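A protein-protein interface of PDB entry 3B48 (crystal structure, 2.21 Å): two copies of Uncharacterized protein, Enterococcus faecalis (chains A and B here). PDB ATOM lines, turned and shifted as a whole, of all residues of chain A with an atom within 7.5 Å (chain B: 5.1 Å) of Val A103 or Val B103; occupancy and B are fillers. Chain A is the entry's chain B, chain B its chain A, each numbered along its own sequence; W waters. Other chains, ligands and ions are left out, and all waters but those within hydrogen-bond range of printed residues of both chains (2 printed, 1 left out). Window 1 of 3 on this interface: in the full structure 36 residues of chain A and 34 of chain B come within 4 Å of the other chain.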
ATOM      1  N   LEU A  10      12.997  20.004  -4.836  1.00  0.00           N
ATOM      2  CA  LEU A  10      12.541  19.820  -6.198  1.00  0.00           C
ATOM      3  C   LEU A  10      13.322  20.762  -7.107  1.00  0.00           C
ATOM      4  O   LEU A  10      13.109  21.984  -7.073  1.00  0.00           O
ATOM      5  CB  LEU A  10      11.040  20.169  -6.302  1.00  0.00           C
ATOM      6  CG  LEU A  10      10.069  19.463  -5.335  1.00  0.00           C
ATOM      7  CD1 LEU A  10       8.713  20.139  -5.427  1.00  0.00           C
ATOM      8  CD2 LEU A  10       9.956  18.041  -5.752  1.00  0.00           C
ATOM      9  N   SER A  12      14.495  21.864 -11.067  1.00  0.00           N
ATOM     10  CA  SER A  12      14.069  21.791 -12.451  1.00  0.00           C
ATOM     11  C   SER A  12      14.579  23.025 -13.132  1.00  0.00           C
ATOM     12  O   SER A  12      14.938  23.956 -12.449  1.00  0.00           O
ATOM     13  CB  SER A  12      12.526  21.738 -12.516  1.00  0.00           C
ATOM     14  OG  SER A  12      12.044  21.623 -13.845  1.00  0.00           O
ATOM     15  N   ILE A  17       6.986  24.086 -12.921  1.00  0.00           N
ATOM     16  CA  ILE A  17       6.918  22.651 -12.573  1.00  0.00           C
ATOM     17  C   ILE A  17       7.050  22.448 -11.049  1.00  0.00           C
ATOM     18  O   ILE A  17       6.154  21.867 -10.425  1.00  0.00           O
ATOM     19  CB  ILE A  17       7.958  21.769 -13.359  1.00  0.00           C
ATOM     20  CG1 ILE A  17       7.623  21.746 -14.850  1.00  0.00           C
ATOM     21  CG2 ILE A  17       8.013  20.367 -12.776  1.00  0.00           C
ATOM     22  CD1 ILE A  17       8.630  21.004 -15.746  1.00  0.00           C
ATOM     23  N   GLY A  20       4.189  23.865  -9.085  1.00  0.00           N
ATOM     24  CA  GLY A  20       3.032  23.023  -9.374  1.00  0.00           C
ATOM     25  C   GLY A  20       3.039  21.725  -8.605  1.00  0.00           C
ATOM     26  O   GLY A  20       2.001  21.301  -8.075  1.00  0.00           O
ATOM     27  N   ILE A  21       4.210  21.092  -8.527  1.00  0.00           N
ATOM     28  CA  ILE A  21       4.370  19.842  -7.748  1.00  0.00           C
ATOM     29  C   ILE A  21       4.066  20.094  -6.268  1.00  0.00           C
ATOM     30  O   ILE A  21       3.310  19.347  -5.646  1.00  0.00           O
ATOM     31  CB  ILE A  21       5.789  19.292  -7.829  1.00  0.00           C
ATOM     32  CG1 ILE A  21       6.147  18.810  -9.231  1.00  0.00           C
ATOM     33  CG2 ILE A  21       5.995  18.139  -6.842  1.00  0.00           C
ATOM     34  CD1 ILE A  21       7.629  18.397  -9.295  1.00  0.00           C
ATOM     35  N   MET A  24       0.434  20.847  -5.671  1.00  0.00           N
ATOM     36  CA  MET A  24      -0.360  19.628  -5.912  1.00  0.00           C
ATOM     37  C   MET A  24      -0.268  18.654  -4.756  1.00  0.00           C
ATOM     38  O   MET A  24      -1.269  18.201  -4.233  1.00  0.00           O
ATOM     39  CB  MET A  24       0.057  18.941  -7.205  1.00  0.00           C
ATOM     40  CG  MET A  24      -0.847  17.787  -7.588  1.00  0.00           C
ATOM     41  SD  MET A  24      -0.230  16.853  -9.189  1.00  0.00           S
ATOM     42  CE  MET A  24       1.476  16.173  -8.485  1.00  0.00           C
ATOM     43  N   ILE A  25       0.945  18.340  -4.347  1.00  0.00           N
ATOM     44  CA  ILE A  25       1.141  17.477  -3.202  1.00  0.00           C
ATOM     45  C   ILE A  25       0.484  18.039  -1.912  1.00  0.00           C
ATOM     46  O   ILE A  25      -0.252  17.333  -1.227  1.00  0.00           O
ATOM     47  CB  ILE A  25       2.633  17.259  -2.986  1.00  0.00           C
ATOM     48  CG1 ILE A  25       3.187  16.392  -4.121  1.00  0.00           C
ATOM     49  CG2 ILE A  25       2.879  16.660  -1.629  1.00  0.00           C
ATOM     50  CD1 ILE A  25       4.624  16.131  -4.003  1.00  0.00           C
ATOM     51  N   PHE A  70      15.253  15.724  -5.653  1.00  0.00           N
ATOM     52  CA  PHE A  70      14.717  15.278  -6.930  1.00  0.00           C
ATOM     53  C   PHE A  70      14.979  16.320  -8.049  1.00  0.00           C
ATOM     54  O   PHE A  70      14.839  17.524  -7.835  1.00  0.00           O
ATOM     55  CB  PHE A  70      13.212  14.996  -6.843  1.00  0.00           C
ATOM     56  CG  PHE A  70      12.834  14.060  -5.747  1.00  0.00           C
ATOM     57  CD1 PHE A  70      12.427  12.762  -6.034  1.00  0.00           C
ATOM     58  CD2 PHE A  70      12.902  14.457  -4.413  1.00  0.00           C
ATOM     59  CE1 PHE A  70      12.094  11.889  -5.015  1.00  0.00           C
ATOM     60  CE2 PHE A  70      12.539  13.579  -3.394  1.00  0.00           C
ATOM     61  CZ  PHE A  70      12.152  12.301  -3.693  1.00  0.00           C
ATOM     62  N   ALA A  71      15.381  15.839  -9.222  1.00  0.00           N
ATOM     63  CA  ALA A  71      15.549  16.687 -10.411  1.00  0.00           C
ATOM     64  C   ALA A  71      14.870  16.013 -11.595  1.00  0.00           C
ATOM     65  O   ALA A  71      14.625  14.797 -11.586  1.00  0.00           O
ATOM     66  CB  ALA A  71      17.030  16.956 -10.707  1.00  0.00           C
ATOM     67  N   ASP A  72      14.519  16.789 -12.606  1.00  0.00           N
ATOM     68  CA  ASP A  72      14.026  16.156 -13.820  1.00  0.00           C
ATOM     69  C   ASP A  72      15.166  15.883 -14.802  1.00  0.00           C
ATOM     70  O   ASP A  72      15.493  14.735 -15.078  1.00  0.00           O
ATOM     71  CB  ASP A  72      12.891  16.939 -14.462  1.00  0.00           C
ATOM     72  CG  ASP A  72      13.159  18.469 -14.560  1.00  0.00           C
ATOM     73  OD1 ASP A  72      14.327  18.948 -14.463  1.00  0.00           O
ATOM     74  OD2 ASP A  72      12.148  19.190 -14.773  1.00  0.00           O
ATOM     75  N   LEU A  73      15.781  16.940 -15.311  1.00  0.00           N
ATOM     76  CA  LEU A  73      16.579  16.828 -16.503  1.00  0.00           C
ATOM     77  C   LEU A  73      17.689  17.854 -16.552  1.00  0.00           C
ATOM     78  O   LEU A  73      17.589  18.952 -15.968  1.00  0.00           O
ATOM     79  CB  LEU A  73      15.690  17.074 -17.740  1.00  0.00           C
ATOM     80  CG  LEU A  73      14.440  16.234 -18.082  1.00  0.00           C
ATOM     81  CD1 LEU A  73      13.478  17.113 -18.797  1.00  0.00           C
ATOM     82  CD2 LEU A  73      14.779  14.980 -18.916  1.00  0.00           C
ATOM     83  N   ALA A 100      15.065   8.913  -9.009  1.00  0.00           N
ATOM     84  CA  ALA A 100      13.620   8.740  -9.165  1.00  0.00           C
ATOM     85  C   ALA A 100      13.064   9.868 -10.023  1.00  0.00           C
ATOM     86  O   ALA A 100      13.633  10.962 -10.030  1.00  0.00           O
ATOM     87  CB  ALA A 100      12.926   8.730  -7.776  1.00  0.00           C
ATOM     88  N   PRO A 101      11.936   9.621 -10.728  1.00  0.00           N
ATOM     89  CA  PRO A 101      11.403  10.721 -11.512  1.00  0.00           C
ATOM     90  C   PRO A 101      10.894  11.814 -10.599  1.00  0.00           C
ATOM     91  O   PRO A 101      10.506  11.537  -9.459  1.00  0.00           O
ATOM     92  CB  PRO A 101      10.268  10.096 -12.325  1.00  0.00           C
ATOM     93  CG  PRO A 101       9.927   8.829 -11.664  1.00  0.00           C
ATOM     94  CD  PRO A 101      11.106   8.405 -10.826  1.00  0.00           C
ATOM     95  N   LEU A 102      10.931  13.046 -11.116  1.00  0.00           N
ATOM     96  CA  LEU A 102      10.658  14.234 -10.363  1.00  0.00           C
ATOM     97  C   LEU A 102       9.260  14.272  -9.675  1.00  0.00           C
ATOM     98  O   LEU A 102       9.188  14.374  -8.432  1.00  0.00           O
ATOM     99  CB  LEU A 102      10.895  15.483 -11.241  1.00  0.00           C
ATOM    100  CG  LEU A 102      10.629  16.835 -10.577  1.00  0.00           C
ATOM    101  CD1 LEU A 102      11.543  17.129  -9.339  1.00  0.00           C
ATOM    102  CD2 LEU A 102      10.690  17.964 -11.562  1.00  0.00           C
ATOM    103  N   VAL A 103       8.178  14.242 -10.465  1.00  0.00           N
ATOM    104  CA  VAL A 103       6.820  14.329  -9.902  1.00  0.00           C
ATOM    105  C   VAL A 103       6.489  13.088  -9.047  1.00  0.00           C
ATOM    106  O   VAL A 103       6.186  13.193  -7.840  1.00  0.00           O
ATOM    107  CB  VAL A 103       5.718  14.525 -11.008  1.00  0.00           C
ATOM    108  CG1 VAL A 103       4.303  14.577 -10.353  1.00  0.00           C
ATOM    109  CG2 VAL A 103       5.976  15.795 -11.826  1.00  0.00           C
ATOM    110  N   GLU A 104       6.572  11.927  -9.690  1.00  0.00           N
ATOM    111  CA  GLU A 104       6.198  10.675  -9.080  1.00  0.00           C
ATOM    112  C   GLU A 104       7.095  10.246  -7.930  1.00  0.00           C
ATOM    113  O   GLU A 104       6.597   9.773  -6.930  1.00  0.00           O
ATOM    114  CB  GLU A 104       6.058   9.569 -10.127  1.00  0.00           C
ATOM    115  CG  GLU A 104       5.031   9.889 -11.246  1.00  0.00           C
ATOM    116  CD  GLU A 104       5.666  10.590 -12.469  1.00  0.00           C
ATOM    117  OE1 GLU A 104       6.770  11.185 -12.370  1.00  0.00           O
ATOM    118  OE2 GLU A 104       5.059  10.532 -13.542  1.00  0.00           O
ATOM    119  N   GLY A 105       8.408  10.405  -8.057  1.00  0.00           N
ATOM    120  CA  GLY A 105       9.318  10.162  -6.921  1.00  0.00           C
ATOM    121  C   GLY A 105       8.979  11.003  -5.697  1.00  0.00           C
ATOM    122  O   GLY A 105       8.767  10.472  -4.597  1.00  0.00           O
ATOM    123  N   ALA A 106       8.874  12.317  -5.896  1.00  0.00           N
ATOM    124  CA  ALA A 106       8.572  13.245  -4.784  1.00  0.00           C
ATOM    125  C   ALA A 106       7.246  12.898  -4.071  1.00  0.00           C
ATOM    126  O   ALA A 106       7.161  12.896  -2.827  1.00  0.00           O
ATOM    127  CB  ALA A 106       8.555  14.682  -5.309  1.00  0.00           C
ATOM    128  N   PHE A 107       6.214  12.598  -4.862  1.00  0.00           N
ATOM    129  CA  PHE A 107       4.902  12.317  -4.313  1.00  0.00           C
ATOM    130  C   PHE A 107       4.995  11.042  -3.496  1.00  0.00           C
ATOM    131  O   PHE A 107       4.459  10.983  -2.389  1.00  0.00           O
ATOM    132  CB  PHE A 107       3.802  12.212  -5.406  1.00  0.00           C
ATOM    133  CG  PHE A 107       2.486  11.649  -4.895  1.00  0.00           C
ATOM    134  CD1 PHE A 107       1.539  12.479  -4.270  1.00  0.00           C
ATOM    135  CD2 PHE A 107       2.215  10.287  -4.986  1.00  0.00           C
ATOM    136  CE1 PHE A 107       0.355  11.948  -3.761  1.00  0.00           C
ATOM    137  CE2 PHE A 107       0.996   9.763  -4.506  1.00  0.00           C
ATOM    138  CZ  PHE A 107       0.078  10.608  -3.894  1.00  0.00           C
ATOM    139  N   ALA A 108       5.656  10.023  -4.061  1.00  0.00           N
ATOM    140  CA  ALA A 108       5.915   8.761  -3.353  1.00  0.00           C
ATOM    141  C   ALA A 108       6.732   8.995  -2.065  1.00  0.00           C
ATOM    142  O   ALA A 108       6.319   8.560  -0.982  1.00  0.00           O
ATOM    143  CB  ALA A 108       6.603   7.784  -4.247  1.00  0.00           C
ATOM    144  N   SER A 109       7.863   9.710  -2.147  1.00  0.00           N
ATOM    145  CA  SER A 109       8.565  10.069  -0.901  1.00  0.00           C
ATOM    146  C   SER A 109       7.624  10.749   0.093  1.00  0.00           C
ATOM    147  O   SER A 109       7.584  10.372   1.231  1.00  0.00           O
ATOM    148  CB  SER A 109       9.820  10.913  -1.158  1.00  0.00           C
ATOM    149  OG  SER A 109      10.837  10.079  -1.685  1.00  0.00           O
ATOM    150  N   ALA A 129       8.900   4.687  -8.468  1.00  0.00           N
ATOM    151  CA  ALA A 129       7.669   5.500  -8.787  1.00  0.00           C
ATOM    152  C   ALA A 129       7.111   5.721 -10.234  1.00  0.00           C
ATOM    153  O   ALA A 129       5.878   5.802 -10.434  1.00  0.00           O
ATOM    154  CB  ALA A 129       7.752   6.852  -8.076  1.00  0.00           C
ATOM    155  N   LYS A 132       2.962   3.120 -14.456  1.00  0.00           N
ATOM    156  CA  LYS A 132       1.527   3.375 -14.384  1.00  0.00           C
ATOM    157  C   LYS A 132       0.727   2.097 -14.634  1.00  0.00           C
ATOM    158  O   LYS A 132      -0.496   2.107 -14.488  1.00  0.00           O
ATOM    159  CB  LYS A 132       1.124   4.433 -15.436  1.00  0.00           C
ATOM    160  CG  LYS A 132       2.160   5.573 -15.742  1.00  0.00           C
ATOM    161  CD  LYS A 132       2.146   6.601 -14.681  1.00  0.00           C
ATOM    162  CE  LYS A 132       3.425   7.381 -14.626  1.00  0.00           C
ATOM    163  NZ  LYS A 132       3.617   7.780 -13.239  1.00  0.00           N
ATOM    164  N   ILE B  17       2.008  22.260 -13.687  1.00  0.00           N
ATOM    165  CA  ILE B  17       2.914  21.189 -14.113  1.00  0.00           C
ATOM    166  C   ILE B  17       2.867  20.956 -15.628  1.00  0.00           C
ATOM    167  O   ILE B  17       3.914  21.028 -16.285  1.00  0.00           O
ATOM    168  CB  ILE B  17       2.680  19.894 -13.300  1.00  0.00           C
ATOM    169  CG1 ILE B  17       3.090  20.116 -11.843  1.00  0.00           C
ATOM    170  CG2 ILE B  17       3.469  18.708 -13.882  1.00  0.00           C
ATOM    171  CD1 ILE B  17       2.733  18.922 -10.911  1.00  0.00           C
ATOM    172  N   ILE B  21       5.803  21.914 -18.135  1.00  0.00           N
ATOM    173  CA  ILE B  21       6.450  20.899 -18.989  1.00  0.00           C
ATOM    174  C   ILE B  21       6.397  21.287 -20.481  1.00  0.00           C
ATOM    175  O   ILE B  21       7.404  21.204 -21.180  1.00  0.00           O
ATOM    176  CB  ILE B  21       5.786  19.528 -18.862  1.00  0.00           C
ATOM    177  CG1 ILE B  21       6.025  18.906 -17.485  1.00  0.00           C
ATOM    178  CG2 ILE B  21       6.262  18.559 -19.994  1.00  0.00           C
ATOM    179  CD1 ILE B  21       4.981  17.828 -17.196  1.00  0.00           C
ATOM    180  N   MET B  24       8.709  24.155 -21.116  1.00  0.00           N
ATOM    181  CA  MET B  24      10.094  23.753 -21.033  1.00  0.00           C
ATOM    182  C   MET B  24      10.539  22.978 -22.273  1.00  0.00           C
ATOM    183  O   MET B  24      11.621  23.218 -22.783  1.00  0.00           O
ATOM    184  CB  MET B  24      10.324  22.937 -19.778  1.00  0.00           C
ATOM    185  CG  MET B  24      11.714  23.072 -19.176  1.00  0.00           C
ATOM    186  SD  MET B  24      11.883  21.739 -17.738  1.00  0.00           S
ATOM    187  CE  MET B  24      11.221  20.125 -18.670  1.00  0.00           C
ATOM    188  N   ASP B  72       0.723  11.628 -14.396  1.00  0.00           N
ATOM    189  CA  ASP B  72       1.555  11.469 -13.203  1.00  0.00           C
ATOM    190  C   ASP B  72       0.989  10.505 -12.168  1.00  0.00           C
ATOM    191  O   ASP B  72       1.499   9.405 -12.026  1.00  0.00           O
ATOM    192  CB  ASP B  72       1.975  12.807 -12.550  1.00  0.00           C
ATOM    193  CG  ASP B  72       0.829  13.808 -12.425  1.00  0.00           C
ATOM    194  OD1 ASP B  72      -0.354  13.398 -12.497  1.00  0.00           O
ATOM    195  OD2 ASP B  72       1.119  15.012 -12.246  1.00  0.00           O
ATOM    196  N   LEU B  73      -0.055  10.920 -11.466  1.00  0.00           N
ATOM    197  CA  LEU B  73      -0.534  10.175 -10.318  1.00  0.00           C
ATOM    198  C   LEU B  73      -1.815   9.405 -10.633  1.00  0.00           C
ATOM    199  O   LEU B  73      -2.252   9.390 -11.793  1.00  0.00           O
ATOM    200  CB  LEU B  73      -0.645  11.095  -9.094  1.00  0.00           C
ATOM    201  CG  LEU B  73       0.608  11.945  -8.776  1.00  0.00           C
ATOM    202  CD1 LEU B  73       0.300  12.815  -7.580  1.00  0.00           C
ATOM    203  CD2 LEU B  73       1.913  11.131  -8.538  1.00  0.00           C
ATOM    204  N   PRO B 101       7.601   8.321 -16.680  1.00  0.00           N
ATOM    205  CA  PRO B 101       7.432   9.496 -15.815  1.00  0.00           C
ATOM    206  C   PRO B 101       6.901  10.700 -16.590  1.00  0.00           C
ATOM    207  O   PRO B 101       7.357  10.973 -17.716  1.00  0.00           O
ATOM    208  CB  PRO B 101       8.848   9.811 -15.334  1.00  0.00           C
ATOM    209  CG  PRO B 101       9.765   9.116 -16.284  1.00  0.00           C
ATOM    210  CD  PRO B 101       9.024   7.929 -16.804  1.00  0.00           C
ATOM    211  N   LEU B 102       5.990  11.436 -15.977  1.00  0.00           N
ATOM    212  CA  LEU B 102       5.343  12.539 -16.671  1.00  0.00           C
ATOM    213  C   LEU B 102       6.323  13.542 -17.285  1.00  0.00           C
ATOM    214  O   LEU B 102       6.199  13.861 -18.453  1.00  0.00           O
ATOM    215  CB  LEU B 102       4.319  13.244 -15.770  1.00  0.00           C
ATOM    216  CG  LEU B 102       3.723  14.549 -16.309  1.00  0.00           C
ATOM    217  CD1 LEU B 102       2.782  14.347 -17.553  1.00  0.00           C
ATOM    218  CD2 LEU B 102       3.001  15.193 -15.206  1.00  0.00           C
ATOM    219  N   VAL B 103       7.309  14.008 -16.525  1.00  0.00           N
ATOM    220  CA  VAL B 103       8.151  15.105 -16.992  1.00  0.00           C
ATOM    221  C   VAL B 103       9.264  14.597 -17.907  1.00  0.00           C
ATOM    222  O   VAL B 103       9.331  14.980 -19.061  1.00  0.00           O
ATOM    223  CB  VAL B 103       8.753  15.920 -15.843  1.00  0.00           C
ATOM    224  CG1 VAL B 103       9.754  16.959 -16.425  1.00  0.00           C
ATOM    225  CG2 VAL B 103       7.641  16.574 -14.947  1.00  0.00           C
ATOM    226  N   GLU B 104      10.116  13.727 -17.369  1.00  0.00           N
ATOM    227  CA  GLU B 104      11.225  13.108 -18.096  1.00  0.00           C
ATOM    228  C   GLU B 104      10.749  12.234 -19.258  1.00  0.00           C
ATOM    229  O   GLU B 104      11.391  12.158 -20.316  1.00  0.00           O
ATOM    230  CB  GLU B 104      12.093  12.295 -17.123  1.00  0.00           C
ATOM    231  CG  GLU B 104      12.637  13.116 -15.904  1.00  0.00           C
ATOM    232  CD  GLU B 104      11.829  12.928 -14.602  1.00  0.00           C
ATOM    233  OE1 GLU B 104      10.590  12.719 -14.647  1.00  0.00           O
ATOM    234  OE2 GLU B 104      12.450  12.975 -13.518  1.00  0.00           O
ATOM    235  N   GLY B 105       9.597  11.588 -19.073  1.00  0.00           N
ATOM    236  CA  GLY B 105       9.022  10.733 -20.116  1.00  0.00           C
ATOM    237  C   GLY B 105       8.661  11.607 -21.290  1.00  0.00           C
ATOM    238  O   GLY B 105       9.033  11.302 -22.422  1.00  0.00           O
ATOM    239  N   ALA B 106       7.962  12.718 -21.025  1.00  0.00           N
ATOM    240  CA  ALA B 106       7.503  13.583 -22.109  1.00  0.00           C
ATOM    241  C   ALA B 106       8.643  14.221 -22.891  1.00  0.00           C
ATOM    242  O   ALA B 106       8.543  14.404 -24.110  1.00  0.00           O
ATOM    243  CB  ALA B 106       6.580  14.629 -21.604  1.00  0.00           C
ATOM    244  N   PHE B 107       9.692  14.612 -22.170  1.00  0.00           N
ATOM    245  CA  PHE B 107      10.861  15.247 -22.756  1.00  0.00           C
ATOM    246  C   PHE B 107      11.587  14.251 -23.644  1.00  0.00           C
ATOM    247  O   PHE B 107      11.936  14.573 -24.772  1.00  0.00           O
ATOM    248  CB  PHE B 107      11.801  15.790 -21.669  1.00  0.00           C
ATOM    249  CG  PHE B 107      12.986  16.578 -22.213  1.00  0.00           C
ATOM    250  CD1 PHE B 107      12.848  17.915 -22.578  1.00  0.00           C
ATOM    251  CD2 PHE B 107      14.245  15.975 -22.353  1.00  0.00           C
ATOM    252  CE1 PHE B 107      13.958  18.658 -23.092  1.00  0.00           C
ATOM    253  CE2 PHE B 107      15.355  16.695 -22.860  1.00  0.00           C
ATOM    254  CZ  PHE B 107      15.203  18.051 -23.231  1.00  0.00           C
HETATM  255  O   HOH W   1      -2.038  14.532 -10.865  1.00  0.00           O
HETATM  256  O   HOH W   2       8.213  13.166 -13.474  1.00  0.00           O
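The backbone carbonyl oxygen (O) of Asp B72 sits at hydrogen-bond distance from the side-chain amino group (NZ) of Lys A132.
The backbone NH (N) of Leu B102 sits at hydrogen-bond distance from the side-chain carboxylate (OE2) of Glu A104, 2.8 Å away.
OE2 of Glu B104 lies within hydrogen-bond range of N of Leu A102 (2.8 Å).
O of Ala A71 lies close to OE2 of Glu B104 (3.4 Å).
OG of Ser A12 lies within hydrogen-bond range of OD2 of Asp A72 (2.6 Å).
OE2 of Glu A104 lies within salt-bridge range of NZ of Lys A132, 3.1 Å away.
Among the printed residues, pairs that only touch across the chains: Pro A101 with Glu B104 (3.2 Å), Pro A101 with Pro B101 (3.3 Å), Asp A72 with Glu B104 (3.4 Å), Glu A104 with Pro B101 (3.4 Å), Leu A73 with Phe B107 (3.5 Å), Ile A21 with Ile B17 (3.5 Å), Phe A107 with Leu B73 (3.6 Å), Gly A20 with Ile B17 (3.6 Å), Val A103 with Val B103 (3.6 Å), Glu A104 with Asp B72 (3.6 Å), Val A103 with Asp B72 (3.7 Å), Asp A72 with Val B103 (3.7 Å), Met A24 with Leu B73 (3.7 Å), Ile A17 with Ile B21 (3.8 Å), Leu A73 with Met B24 (3.8 Å), Ile A17 with Ile B17 (3.8 Å), Met A24 with Asp B72 (3.8 Å), Met A24 with Ile B17 (3.9 Å), Ile A17 with Met B24 (3.9 Å), Ser A12 with Met B24 (3.9 Å) and Asp A72 with Met B24 (3.9 Å).
Val A103 touches just these residues of chain B: Asp B72 (3.7 Å) and Val B103 (3.6 Å).
Val B103 touches just these residues of chain A: Asp A72 (3.7 Å) and Val A103 (3.6 Å).
Of the printed residues of chain A, Glu B104 touches Ala A71 (3.4 Å), Asp A72 (3.4 Å), Pro A101 (3.2 Å) and Leu A102 (2.8 Å).
Of the printed residues of chain B, Glu A104 touches Asp B72, Pro B101 and Leu B102.
The nearest residue of chain B that does not touch Val A103 is Ile B17 (4.4 Å).
The nearest residue of chain A that does not touch Val B103 is Ile A17 (4.3 Å).
The nearest printed residue of chain B that does not touch Ile A17 is Val B103 (4.3 Å).
Printed residues of chain A that touch a printed residue of chain B: Ser A12, Ile A17, Gly A20, Ile A21, Met A24, Ala A71, Asp A72, Leu A73, Pro A101, Leu A102, Val A103, Glu A104, Phe A107 and Lys A132.
Hydrophobic or aromatic side chains of chain A that line the printed part of chain B: Ile A17, Ile A21, Met A24, Leu A73, Pro A101, Leu A102, Val A103 and Phe A107.
Of the 12 printed residues of chain B, 10 touch a printed residue of chain A.
Hydrophobic or aromatic side chains of chain B within 4 Å of the printed part of chain A: Ile B17, Ile B21, Met B24, Leu B73, Pro B101, Leu B102, Val B103 and Phe B107.
Among the printed residues, 25 pairs touch across the chains.
Met A24 touches Asp B72, and with the chains exchanged Asp A72 touches Met B24.
Met A24 touches Leu B73, and with the chains exchanged Leu A73 touches Met B24.
Leu A73 touches Phe B107, and with the chains exchanged Phe A107 touches Leu B73.
Leu A102 touches Glu B104, and with the chains exchanged Glu A104 touches Leu B102.
12 positions are printed for both chains.
Of the 25 pairs that touch across the chains among the printed residues, 21 have their exchanged pair printed and touching as well.
Water W1 lies within hydrogen-bond range of OD1 of Asp B72 and SD of Met A24.
Water W2 lies within hydrogen-bond range of the side-chain carboxylate of Glu A104 (2.7 Å), the side-chain carboxylate of Glu B104 (2.7 Å), the backbone NH of Val A103 (3.2 Å) and the backbone NH of Val B103 (3.3 Å).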
